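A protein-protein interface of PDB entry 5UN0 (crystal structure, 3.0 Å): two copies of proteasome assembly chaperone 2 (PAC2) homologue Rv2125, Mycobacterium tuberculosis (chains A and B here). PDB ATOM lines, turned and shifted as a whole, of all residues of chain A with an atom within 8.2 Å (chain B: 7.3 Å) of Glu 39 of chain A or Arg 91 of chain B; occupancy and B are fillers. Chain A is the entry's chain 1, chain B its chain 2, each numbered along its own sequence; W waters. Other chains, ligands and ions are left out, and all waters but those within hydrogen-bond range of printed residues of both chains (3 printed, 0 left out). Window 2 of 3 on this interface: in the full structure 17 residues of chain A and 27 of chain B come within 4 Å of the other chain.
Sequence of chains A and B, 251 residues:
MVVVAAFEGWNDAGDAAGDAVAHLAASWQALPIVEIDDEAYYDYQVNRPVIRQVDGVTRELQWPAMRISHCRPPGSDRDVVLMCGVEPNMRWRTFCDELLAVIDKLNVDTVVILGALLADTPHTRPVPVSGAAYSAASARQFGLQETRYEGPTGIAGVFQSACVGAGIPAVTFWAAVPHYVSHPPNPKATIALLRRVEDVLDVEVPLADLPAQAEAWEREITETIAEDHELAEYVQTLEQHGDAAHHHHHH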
ATOM      1  N   ILE A  36       0.394 -27.140   4.087  1.00  0.00           N
ATOM      2  CA  ILE A  36      -0.697 -26.151   3.997  1.00  0.00           C
ATOM      3  C   ILE A  36      -0.349 -24.898   4.800  1.00  0.00           C
ATOM      4  O   ILE A  36      -0.459 -24.848   6.033  1.00  0.00           O
ATOM      5  CB  ILE A  36      -2.057 -26.731   4.407  1.00  0.00           C
ATOM      6  CG1 ILE A  36      -2.464 -27.823   3.427  1.00  0.00           C
ATOM      7  CG2 ILE A  36      -3.132 -25.655   4.397  1.00  0.00           C
ATOM      8  CD1 ILE A  36      -3.779 -28.504   3.771  1.00  0.00           C
ATOM      9  N   ASP A  37       0.030 -23.879   4.034  1.00  0.00           N
ATOM     10  CA  ASP A  37       0.698 -22.661   4.491  1.00  0.00           C
ATOM     11  C   ASP A  37      -0.282 -21.495   4.570  1.00  0.00           C
ATOM     12  O   ASP A  37       0.065 -20.419   5.050  1.00  0.00           O
ATOM     13  CB  ASP A  37       1.772 -22.323   3.451  1.00  0.00           C
ATOM     14  CG  ASP A  37       2.752 -21.292   3.921  1.00  0.00           C
ATOM     15  OD1 ASP A  37       3.219 -21.366   5.086  1.00  0.00           O
ATOM     16  OD2 ASP A  37       3.071 -20.400   3.105  1.00  0.00           O
ATOM     17  N   ASP A  38      -1.511 -21.721   4.111  1.00  0.00           N
ATOM     18  CA  ASP A  38      -2.403 -20.633   3.751  1.00  0.00           C
ATOM     19  C   ASP A  38      -2.723 -19.685   4.893  1.00  0.00           C
ATOM     20  O   ASP A  38      -3.008 -20.085   6.017  1.00  0.00           O
ATOM     21  CB  ASP A  38      -3.700 -21.163   3.166  1.00  0.00           C
ATOM     22  CG  ASP A  38      -4.334 -20.192   2.203  1.00  0.00           C
ATOM     23  OD1 ASP A  38      -4.397 -18.989   2.497  1.00  0.00           O
ATOM     24  OD2 ASP A  38      -4.770 -20.642   1.132  1.00  0.00           O
ATOM     25  N   GLU A  39      -2.683 -18.405   4.553  1.00  0.00           N
ATOM     26  CA  GLU A  39      -2.932 -17.320   5.496  1.00  0.00           C
ATOM     27  C   GLU A  39      -4.444 -17.098   5.711  1.00  0.00           C
ATOM     28  O   GLU A  39      -4.848 -16.307   6.565  1.00  0.00           O
ATOM     29  CB  GLU A  39      -2.188 -16.039   5.046  1.00  0.00           C
ATOM     30  CG  GLU A  39      -2.805 -15.304   3.867  1.00  0.00           C
ATOM     31  CD  GLU A  39      -1.950 -14.145   3.364  1.00  0.00           C
ATOM     32  OE1 GLU A  39      -0.994 -13.719   4.074  1.00  0.00           O
ATOM     33  OE2 GLU A  39      -2.252 -13.652   2.245  1.00  0.00           O
ATOM     34  N   ALA A  40      -5.267 -17.795   4.938  1.00  0.00           N
ATOM     35  CA  ALA A  40      -6.696 -17.862   5.216  1.00  0.00           C
ATOM     36  C   ALA A  40      -6.998 -18.543   6.558  1.00  0.00           C
ATOM     37  O   ALA A  40      -8.041 -18.309   7.140  1.00  0.00           O
ATOM     38  CB  ALA A  40      -7.414 -18.598   4.101  1.00  0.00           C
ATOM     39  N   TYR A  41      -6.098 -19.391   7.027  1.00  0.00           N
ATOM     40  CA  TYR A  41      -6.345 -20.211   8.215  1.00  0.00           C
ATOM     41  C   TYR A  41      -5.725 -19.693   9.514  1.00  0.00           C
ATOM     42  O   TYR A  41      -6.169 -20.091  10.573  1.00  0.00           O
ATOM     43  CB  TYR A  41      -5.876 -21.657   7.951  1.00  0.00           C
ATOM     44  CG  TYR A  41      -6.490 -22.223   6.695  1.00  0.00           C
ATOM     45  CD1 TYR A  41      -7.853 -22.171   6.503  1.00  0.00           C
ATOM     46  CD2 TYR A  41      -5.712 -22.764   5.692  1.00  0.00           C
ATOM     47  CE1 TYR A  41      -8.436 -22.666   5.356  1.00  0.00           C
ATOM     48  CE2 TYR A  41      -6.284 -23.253   4.527  1.00  0.00           C
ATOM     49  CZ  TYR A  41      -7.653 -23.197   4.364  1.00  0.00           C
ATOM     50  OH  TYR A  41      -8.268 -23.672   3.233  1.00  0.00           O
ATOM     51  N   TYR A  42      -4.750 -18.785   9.419  1.00  0.00           N
ATOM     52  CA  TYR A  42      -3.891 -18.423  10.563  1.00  0.00           C
ATOM     53  C   TYR A  42      -3.905 -16.962  11.014  1.00  0.00           C
ATOM     54  O   TYR A  42      -3.689 -16.038  10.210  1.00  0.00           O
ATOM     55  CB  TYR A  42      -2.448 -18.858  10.293  1.00  0.00           C
ATOM     56  CG  TYR A  42      -2.341 -20.352  10.158  1.00  0.00           C
ATOM     57  CD1 TYR A  42      -2.120 -20.964   8.916  1.00  0.00           C
ATOM     58  CD2 TYR A  42      -2.504 -21.171  11.266  1.00  0.00           C
ATOM     59  CE1 TYR A  42      -2.041 -22.346   8.795  1.00  0.00           C
ATOM     60  CE2 TYR A  42      -2.419 -22.546  11.148  1.00  0.00           C
ATOM     61  CZ  TYR A  42      -2.193 -23.126   9.915  1.00  0.00           C
ATOM     62  OH  TYR A  42      -2.128 -24.494   9.860  1.00  0.00           O
ATOM     63  N   ASP A  43      -4.168 -16.793  12.319  1.00  0.00           N
ATOM     64  CA  ASP A  43      -4.045 -15.523  13.067  1.00  0.00           C
ATOM     65  C   ASP A  43      -2.630 -15.524  13.608  1.00  0.00           C
ATOM     66  O   ASP A  43      -2.282 -16.362  14.445  1.00  0.00           O
ATOM     67  CB  ASP A  43      -5.067 -15.462  14.232  1.00  0.00           C
ATOM     68  CG  ASP A  43      -5.093 -14.107  14.980  1.00  0.00           C
ATOM     69  OD1 ASP A  43      -4.036 -13.634  15.435  1.00  0.00           O
ATOM     70  OD2 ASP A  43      -6.200 -13.526  15.149  1.00  0.00           O
ATOM     71  N   TYR A  44      -1.825 -14.574  13.131  1.00  0.00           N
ATOM     72  CA  TYR A  44      -0.388 -14.615  13.344  1.00  0.00           C
ATOM     73  C   TYR A  44       0.088 -13.955  14.632  1.00  0.00           C
ATOM     74  O   TYR A  44       1.248 -14.070  14.984  1.00  0.00           O
ATOM     75  CB  TYR A  44       0.312 -14.010  12.149  1.00  0.00           C
ATOM     76  CG  TYR A  44       0.167 -14.838  10.896  1.00  0.00           C
ATOM     77  CD1 TYR A  44       0.636 -16.137  10.853  1.00  0.00           C
ATOM     78  CD2 TYR A  44      -0.419 -14.315   9.750  1.00  0.00           C
ATOM     79  CE1 TYR A  44       0.512 -16.906   9.712  1.00  0.00           C
ATOM     80  CE2 TYR A  44      -0.544 -15.078   8.591  1.00  0.00           C
ATOM     81  CZ  TYR A  44      -0.076 -16.378   8.574  1.00  0.00           C
ATOM     82  OH  TYR A  44      -0.182 -17.169   7.445  1.00  0.00           O
ATOM     83  N   TRP A  63       6.860 -20.116   8.979  1.00  0.00           N
ATOM     84  CA  TRP A  63       5.435 -19.824   9.124  1.00  0.00           C
ATOM     85  C   TRP A  63       4.623 -21.011   9.638  1.00  0.00           C
ATOM     86  O   TRP A  63       4.819 -22.139   9.184  1.00  0.00           O
ATOM     87  CB  TRP A  63       4.853 -19.416   7.775  1.00  0.00           C
ATOM     88  CG  TRP A  63       5.401 -18.138   7.263  1.00  0.00           C
ATOM     89  CD1 TRP A  63       6.534 -17.968   6.537  1.00  0.00           C
ATOM     90  CD2 TRP A  63       4.837 -16.843   7.443  1.00  0.00           C
ATOM     91  NE1 TRP A  63       6.710 -16.638   6.245  1.00  0.00           N
ATOM     92  CE2 TRP A  63       5.677 -15.928   6.796  1.00  0.00           C
ATOM     93  CE3 TRP A  63       3.693 -16.371   8.075  1.00  0.00           C
ATOM     94  CZ2 TRP A  63       5.416 -14.571   6.774  1.00  0.00           C
ATOM     95  CZ3 TRP A  63       3.437 -15.035   8.056  1.00  0.00           C
ATOM     96  CH2 TRP A  63       4.293 -14.141   7.415  1.00  0.00           C
ATOM     97  N   PRO A  64       3.659 -20.748  10.537  1.00  0.00           N
ATOM     98  CA  PRO A  64       2.801 -21.824  11.001  1.00  0.00           C
ATOM     99  C   PRO A  64       2.093 -22.439   9.823  1.00  0.00           C
ATOM    100  O   PRO A  64       1.769 -21.736   8.868  1.00  0.00           O
ATOM    101  CB  PRO A  64       1.799 -21.116  11.903  1.00  0.00           C
ATOM    102  CG  PRO A  64       1.775 -19.719  11.405  1.00  0.00           C
ATOM    103  CD  PRO A  64       3.174 -19.427  10.976  1.00  0.00           C
ATOM    104  N   MET A  90      -8.992 -20.091  12.019  1.00  0.00           N
ATOM    105  CA  MET A  90     -10.159 -19.694  11.212  1.00  0.00           C
ATOM    106  C   MET A  90     -10.382 -20.533   9.968  1.00  0.00           C
ATOM    107  O   MET A  90      -9.535 -21.324   9.579  1.00  0.00           O
ATOM    108  CB  MET A  90     -10.058 -18.216  10.832  1.00  0.00           C
ATOM    109  CG  MET A  90      -8.678 -17.806  10.386  1.00  0.00           C
ATOM    110  SD  MET A  90      -8.315 -16.071  10.613  1.00  0.00           S
ATOM    111  CE  MET A  90      -8.563 -15.902  12.385  1.00  0.00           C
ATOM    112  N   ARG A  91     -11.545 -20.338   9.363  1.00  0.00           N
ATOM    113  CA  ARG A  91     -11.997 -21.100   8.185  1.00  0.00           C
ATOM    114  C   ARG A  91     -11.835 -22.628   8.329  1.00  0.00           C
ATOM    115  O   ARG A  91     -11.489 -23.324   7.370  1.00  0.00           O
ATOM    116  CB  ARG A  91     -11.342 -20.580   6.901  1.00  0.00           C
ATOM    117  CG  ARG A  91     -11.755 -19.161   6.554  1.00  0.00           C
ATOM    118  CD  ARG A  91     -11.615 -18.883   5.060  1.00  0.00           C
ATOM    119  NE  ARG A  91     -11.913 -17.490   4.699  1.00  0.00           N
ATOM    120  CZ  ARG A  91     -13.137 -16.988   4.490  1.00  0.00           C
ATOM    121  NH1 ARG A  91     -14.213 -17.757   4.624  1.00  0.00           N
ATOM    122  NH2 ARG A  91     -13.293 -15.705   4.161  1.00  0.00           N
ATOM    123  N   ALA B  40      -9.323  -7.030   6.160  1.00  0.00           N
ATOM    124  CA  ALA B  40      -8.559  -8.248   5.890  1.00  0.00           C
ATOM    125  C   ALA B  40      -7.424  -8.482   6.889  1.00  0.00           C
ATOM    126  O   ALA B  40      -7.018  -9.608   7.100  1.00  0.00           O
ATOM    127  CB  ALA B  40      -7.987  -8.203   4.486  1.00  0.00           C
ATOM    128  N   TYR B  41      -6.935  -7.419   7.513  1.00  0.00           N
ATOM    129  CA  TYR B  41      -5.770  -7.493   8.397  1.00  0.00           C
ATOM    130  C   TYR B  41      -6.069  -7.537   9.892  1.00  0.00           C
ATOM    131  O   TYR B  41      -5.214  -7.962  10.647  1.00  0.00           O
ATOM    132  CB  TYR B  41      -4.839  -6.316   8.091  1.00  0.00           C
ATOM    133  CG  TYR B  41      -4.504  -6.252   6.621  1.00  0.00           C
ATOM    134  CD1 TYR B  41      -4.016  -7.361   5.967  1.00  0.00           C
ATOM    135  CD2 TYR B  41      -4.707  -5.097   5.882  1.00  0.00           C
ATOM    136  CE1 TYR B  41      -3.709  -7.320   4.627  1.00  0.00           C
ATOM    137  CE2 TYR B  41      -4.405  -5.049   4.533  1.00  0.00           C
ATOM    138  CZ  TYR B  41      -3.905  -6.173   3.907  1.00  0.00           C
ATOM    139  OH  TYR B  41      -3.602  -6.176   2.568  1.00  0.00           O
ATOM    140  N   TYR B  42      -7.281  -7.140  10.302  1.00  0.00           N
ATOM    141  CA  TYR B  42      -7.594  -6.880  11.731  1.00  0.00           C
ATOM    142  C   TYR B  42      -8.695  -7.726  12.391  1.00  0.00           C
ATOM    143  O   TYR B  42      -9.809  -7.850  11.864  1.00  0.00           O
ATOM    144  CB  TYR B  42      -7.909  -5.404  11.926  1.00  0.00           C
ATOM    145  CG  TYR B  42      -6.718  -4.530  11.588  1.00  0.00           C
ATOM    146  CD1 TYR B  42      -6.694  -3.737  10.436  1.00  0.00           C
ATOM    147  CD2 TYR B  42      -5.612  -4.515  12.406  1.00  0.00           C
ATOM    148  CE1 TYR B  42      -5.600  -2.947  10.125  1.00  0.00           C
ATOM    149  CE2 TYR B  42      -4.525  -3.736  12.101  1.00  0.00           C
ATOM    150  CZ  TYR B  42      -4.524  -2.960  10.963  1.00  0.00           C
ATOM    151  OH  TYR B  42      -3.408  -2.205  10.707  1.00  0.00           O
ATOM    152  N   PRO B  88      -1.095  -5.876  12.651  1.00  0.00           N
ATOM    153  CA  PRO B  88      -2.244  -6.654  12.221  1.00  0.00           C
ATOM    154  C   PRO B  88      -2.290  -8.043  12.843  1.00  0.00           C
ATOM    155  O   PRO B  88      -1.268  -8.551  13.291  1.00  0.00           O
ATOM    156  CB  PRO B  88      -2.043  -6.770  10.704  1.00  0.00           C
ATOM    157  CG  PRO B  88      -0.602  -6.492  10.472  1.00  0.00           C
ATOM    158  CD  PRO B  88      -0.258  -5.471  11.510  1.00  0.00           C
ATOM    159  N   ASN B  89      -3.474  -8.637  12.854  1.00  0.00           N
ATOM    160  CA  ASN B  89      -3.637  -9.997  13.319  1.00  0.00           C
ATOM    161  C   ASN B  89      -3.550 -11.062  12.229  1.00  0.00           C
ATOM    162  O   ASN B  89      -3.470 -12.252  12.541  1.00  0.00           O
ATOM    163  CB  ASN B  89      -4.980 -10.146  14.017  1.00  0.00           C
ATOM    164  CG  ASN B  89      -4.993  -9.505  15.385  1.00  0.00           C
ATOM    165  OD1 ASN B  89      -5.180  -8.309  15.525  1.00  0.00           O
ATOM    166  ND2 ASN B  89      -4.785 -10.322  16.415  1.00  0.00           N
ATOM    167  N   MET B  90      -3.596 -10.658  10.959  1.00  0.00           N
ATOM    168  CA  MET B  90      -3.686 -11.637   9.865  1.00  0.00           C
ATOM    169  C   MET B  90      -3.271 -11.111   8.502  1.00  0.00           C
ATOM    170  O   MET B  90      -3.064  -9.922   8.323  1.00  0.00           O
ATOM    171  CB  MET B  90      -5.097 -12.203   9.803  1.00  0.00           C
ATOM    172  CG  MET B  90      -6.168 -11.145   9.965  1.00  0.00           C
ATOM    173  SD  MET B  90      -7.744 -11.756  10.584  1.00  0.00           S
ATOM    174  CE  MET B  90      -7.224 -12.475  12.142  1.00  0.00           C
ATOM    175  N   ARG B  91      -3.133 -12.034   7.561  1.00  0.00           N
ATOM    176  CA  ARG B  91      -2.662 -11.757   6.196  1.00  0.00           C
ATOM    177  C   ARG B  91      -1.404 -10.876   6.144  1.00  0.00           C
ATOM    178  O   ARG B  91      -1.250 -10.019   5.255  1.00  0.00           O
ATOM    179  CB  ARG B  91      -3.781 -11.165   5.338  1.00  0.00           C
ATOM    180  CG  ARG B  91      -4.919 -12.138   5.097  1.00  0.00           C
ATOM    181  CD  ARG B  91      -5.681 -11.811   3.827  1.00  0.00           C
ATOM    182  NE  ARG B  91      -6.830 -12.699   3.652  1.00  0.00           N
ATOM    183  CZ  ARG B  91      -6.797 -13.922   3.106  1.00  0.00           C
ATOM    184  NH1 ARG B  91      -5.659 -14.435   2.670  1.00  0.00           N
ATOM    185  NH2 ARG B  91      -7.919 -14.641   2.988  1.00  0.00           N
ATOM    186  N   TRP B  92      -0.504 -11.132   7.093  1.00  0.00           N
ATOM    187  CA  TRP B  92       0.803 -10.487   7.164  1.00  0.00           C
ATOM    188  C   TRP B  92       1.515 -10.463   5.812  1.00  0.00           C
ATOM    189  O   TRP B  92       2.002  -9.432   5.380  1.00  0.00           O
ATOM    190  CB  TRP B  92       1.685 -11.216   8.191  1.00  0.00           C
ATOM    191  CG  TRP B  92       1.339 -10.944   9.614  1.00  0.00           C
ATOM    192  CD1 TRP B  92       0.204 -10.385  10.074  1.00  0.00           C
ATOM    193  CD2 TRP B  92       2.137 -11.237  10.764  1.00  0.00           C
ATOM    194  NE1 TRP B  92       0.243 -10.275  11.441  1.00  0.00           N
ATOM    195  CE2 TRP B  92       1.417 -10.809  11.890  1.00  0.00           C
ATOM    196  CE3 TRP B  92       3.383 -11.827  10.952  1.00  0.00           C
ATOM    197  CZ2 TRP B  92       1.899 -10.950  13.189  1.00  0.00           C
ATOM    198  CZ3 TRP B  92       3.867 -11.965  12.243  1.00  0.00           C
ATOM    199  CH2 TRP B  92       3.130 -11.523  13.345  1.00  0.00           C
ATOM    200  N   ARG B  93       1.586 -11.599   5.154  1.00  0.00           N
ATOM    201  CA  ARG B  93       2.247 -11.681   3.834  1.00  0.00           C
ATOM    202  C   ARG B  93       1.749 -10.632   2.825  1.00  0.00           C
ATOM    203  O   ARG B  93       2.548  -9.964   2.180  1.00  0.00           O
ATOM    204  CB  ARG B  93       2.022 -13.069   3.227  1.00  0.00           C
ATOM    205  CG  ARG B  93       3.110 -13.570   2.297  1.00  0.00           C
ATOM    206  CD  ARG B  93       2.910 -15.066   2.037  1.00  0.00           C
ATOM    207  NE  ARG B  93       3.050 -15.871   3.268  1.00  0.00           N
ATOM    208  CZ  ARG B  93       2.147 -16.726   3.767  1.00  0.00           C
ATOM    209  NH1 ARG B  93       0.990 -16.945   3.153  1.00  0.00           N
ATOM    210  NH2 ARG B  93       2.410 -17.380   4.891  1.00  0.00           N
ATOM    211  N   THR B  94       0.433 -10.501   2.721  1.00  0.00           N
ATOM    212  CA  THR B  94      -0.206  -9.556   1.816  1.00  0.00           C
ATOM    213  C   THR B  94      -0.179  -8.109   2.329  1.00  0.00           C
ATOM    214  O   THR B  94      -0.198  -7.159   1.541  1.00  0.00           O
ATOM    215  CB  THR B  94      -1.667  -9.966   1.611  1.00  0.00           C
ATOM    216  OG1 THR B  94      -1.764 -11.394   1.641  1.00  0.00           O
ATOM    217  CG2 THR B  94      -2.187  -9.441   0.280  1.00  0.00           C
ATOM    218  N   PHE B  95      -0.169  -7.969   3.654  1.00  0.00           N
ATOM    219  CA  PHE B  95      -0.005  -6.688   4.336  1.00  0.00           C
ATOM    220  C   PHE B  95       1.343  -6.109   3.966  1.00  0.00           C
ATOM    221  O   PHE B  95       1.458  -4.917   3.660  1.00  0.00           O
ATOM    222  CB  PHE B  95      -0.065  -6.903   5.851  1.00  0.00           C
ATOM    223  CG  PHE B  95       0.136  -5.654   6.680  1.00  0.00           C
ATOM    224  CD1 PHE B  95      -0.950  -4.864   7.057  1.00  0.00           C
ATOM    225  CD2 PHE B  95       1.389  -5.298   7.133  1.00  0.00           C
ATOM    226  CE1 PHE B  95      -0.785  -3.728   7.838  1.00  0.00           C
ATOM    227  CE2 PHE B  95       1.560  -4.164   7.917  1.00  0.00           C
ATOM    228  CZ  PHE B  95       0.471  -3.380   8.270  1.00  0.00           C
ATOM    229  N   CYS B  96       2.364  -6.961   3.996  1.00  0.00           N
ATOM    230  CA  CYS B  96       3.722  -6.543   3.666  1.00  0.00           C
ATOM    231  C   CYS B  96       3.853  -6.214   2.179  1.00  0.00           C
ATOM    232  O   CYS B  96       4.456  -5.197   1.811  1.00  0.00           O
ATOM    233  CB  CYS B  96       4.721  -7.606   4.091  1.00  0.00           C
ATOM    234  SG  CYS B  96       4.896  -7.698   5.890  1.00  0.00           S
ATOM    235  N   ASP B  97       3.264  -7.046   1.324  1.00  0.00           N
ATOM    236  CA  ASP B  97       3.189  -6.748  -0.122  1.00  0.00           C
ATOM    237  C   ASP B  97       2.543  -5.386  -0.389  1.00  0.00           C
ATOM    238  O   ASP B  97       2.987  -4.641  -1.268  1.00  0.00           O
ATOM    239  CB  ASP B  97       2.386  -7.816  -0.865  1.00  0.00           C
ATOM    240  CG  ASP B  97       3.086  -9.165  -0.908  1.00  0.00           C
ATOM    241  OD1 ASP B  97       4.339  -9.225  -0.826  1.00  0.00           O
ATOM    242  OD2 ASP B  97       2.365 -10.183  -1.042  1.00  0.00           O
ATOM    243  N   ILE B 155       5.450  -8.459  13.329  1.00  0.00           N
ATOM    244  CA  ILE B 155       5.344  -7.854  12.005  1.00  0.00           C
ATOM    245  C   ILE B 155       6.600  -7.050  11.644  1.00  0.00           C
ATOM    246  O   ILE B 155       6.988  -6.950  10.468  1.00  0.00           O
ATOM    247  CB  ILE B 155       4.086  -6.972  11.914  1.00  0.00           C
ATOM    248  CG1 ILE B 155       3.813  -6.519  10.476  1.00  0.00           C
ATOM    249  CG2 ILE B 155       4.204  -5.760  12.831  1.00  0.00           C
ATOM    250  CD1 ILE B 155       3.586  -7.654   9.503  1.00  0.00           C
HETATM  251  O   HOH W   1      -1.286 -17.250   1.667  1.00  0.00           O
HETATM  252  O   HOH W   2     -10.494 -16.630   2.270  1.00  0.00           O
HETATM  253  O   HOH W   3       0.669 -18.821   1.346  1.00  0.00           O
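Hydrophobic or aromatic side chains of chain B that line the printed part of chain A: Met 90 and Trp 92.
Of the 13 printed residues of chain A, 6 touch a printed residue of chain B.
Hydrophobic or aromatic side chains of chain A that line the printed part of chain B: Tyr 44, Trp 63 and Met 90.
Among the printed residues, Asp or Glu carboxylates within 4 Å of a Lys or Arg side-chain nitrogen of the other chain: Asp 37 of chain A with Arg 93 of chain B (3.6 Å), Glu 39 of chain A with Arg 91 of chain B (3.5 Å) and Glu 39 of chain A with Arg 93 of chain B (3.9 Å).
Met 90 of chain A touches its own counterpart, Met 90 of chain B.
Of the 12 pairs that touch across the chains among the printed residues, 1 has its exchanged pair printed and touching as well.
Water W3 bridges NH1 of Arg 93 of chain B (2.6 Å) and OD2 of Asp 37 of chain A (3.4 Å).
Water W1 bridges NH1 of Arg 93 of chain B (2.7 Å) and N of Glu 39 of chain A (3.4 Å).
Water W2 lies within hydrogen-bond range of the guanidinium group of Arg 91 of chain A and the guanidinium group of Arg 91 of chain B.
The indole nitrogen of Trp 92 of chain B is in hydrogen-bond range of the backbone carbonyl oxygen of Pro 88 of chain B.
The backbone carbonyl oxygen (O) of Tyr 41 of chain B sits at hydrogen-bond distance from the backbone NH (N) of Met 90 of chain B, at 3.2 Å.
The backbone NH (N) of Met 90 of chain A is in hydrogen-bond range of the backbone carbonyl oxygen (O) of Tyr 41 of chain A, 3.2 Å away.
O of Tyr 41 of chain B is in hydrogen-bond range of N of Asn 89 of chain B (2.9 Å).
The side-chain sulfur of Cys 96 of chain B lies within hydrogen-bond range of the backbone carbonyl oxygen of Trp 92 of chain B, at 3.4 Å.
Among the printed residues, pairs that only touch across the chains: Asp 43 of chain A with Met 90 of chain B (3.3 Å), Tyr 44 of chain A with Trp 92 of chain B (3.4 Å), Trp 63 of chain A with Arg 93 of chain B (3.6 Å), Tyr 44 of chain A with Arg 93 of chain B (3.6 Å), Met 90 of chain A with Met 90 of chain B (3.7 Å) and Trp 63 of chain A with Trp 92 of chain B (3.99 Å).
Of the printed residues of chain B, Glu 39 of chain A touches Arg 91 (3.2 Å), Arg 93 (3.2 Å) and Thr 94 (2.4 Å).
Printed residues of chain B within 4 Å of Met 90 of chain A: Met 90 (3.7 Å).
Of chain A, only Glu 39 (3.2 Å) comes within 4 Å of Arg 91 of chain B.
Of the printed residues of chain A, Thr 94 of chain B touches Glu 39.
The nearest residue of chain A that does not touch Arg 91 of chain B is Ala 40 of chain A (4.1 Å).
The side-chain carboxylate (OE2) of Glu 39 of chain A is in salt-bridge range of the guanidinium group (NH1) of Arg 91 of chain B (3.5 Å).
The side-chain carboxylate (OD2) of Asp 37 of chain A lies within salt-bridge range of the guanidinium group (NH2) of Arg 93 of chain B, 3.6 Å away.
OE1 of Glu 39 of chain A lies within salt-bridge range of NH1 of Arg 93 of chain B.
O of Asn 89 of chain B lies close to OD1 of Asp 43 of chain A (3.3 Å).
The backbone carbonyl oxygen of Asn 89 of chain B sits at hydrogen-bond distance from the backbone NH of Tyr 44 of chain A, 2.9 Å away.
The side-chain hydroxyl (OG1) of Thr 94 of chain B lies close to the side-chain carboxylate (OE1) of Glu 39 of chain A (3.5 Å).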
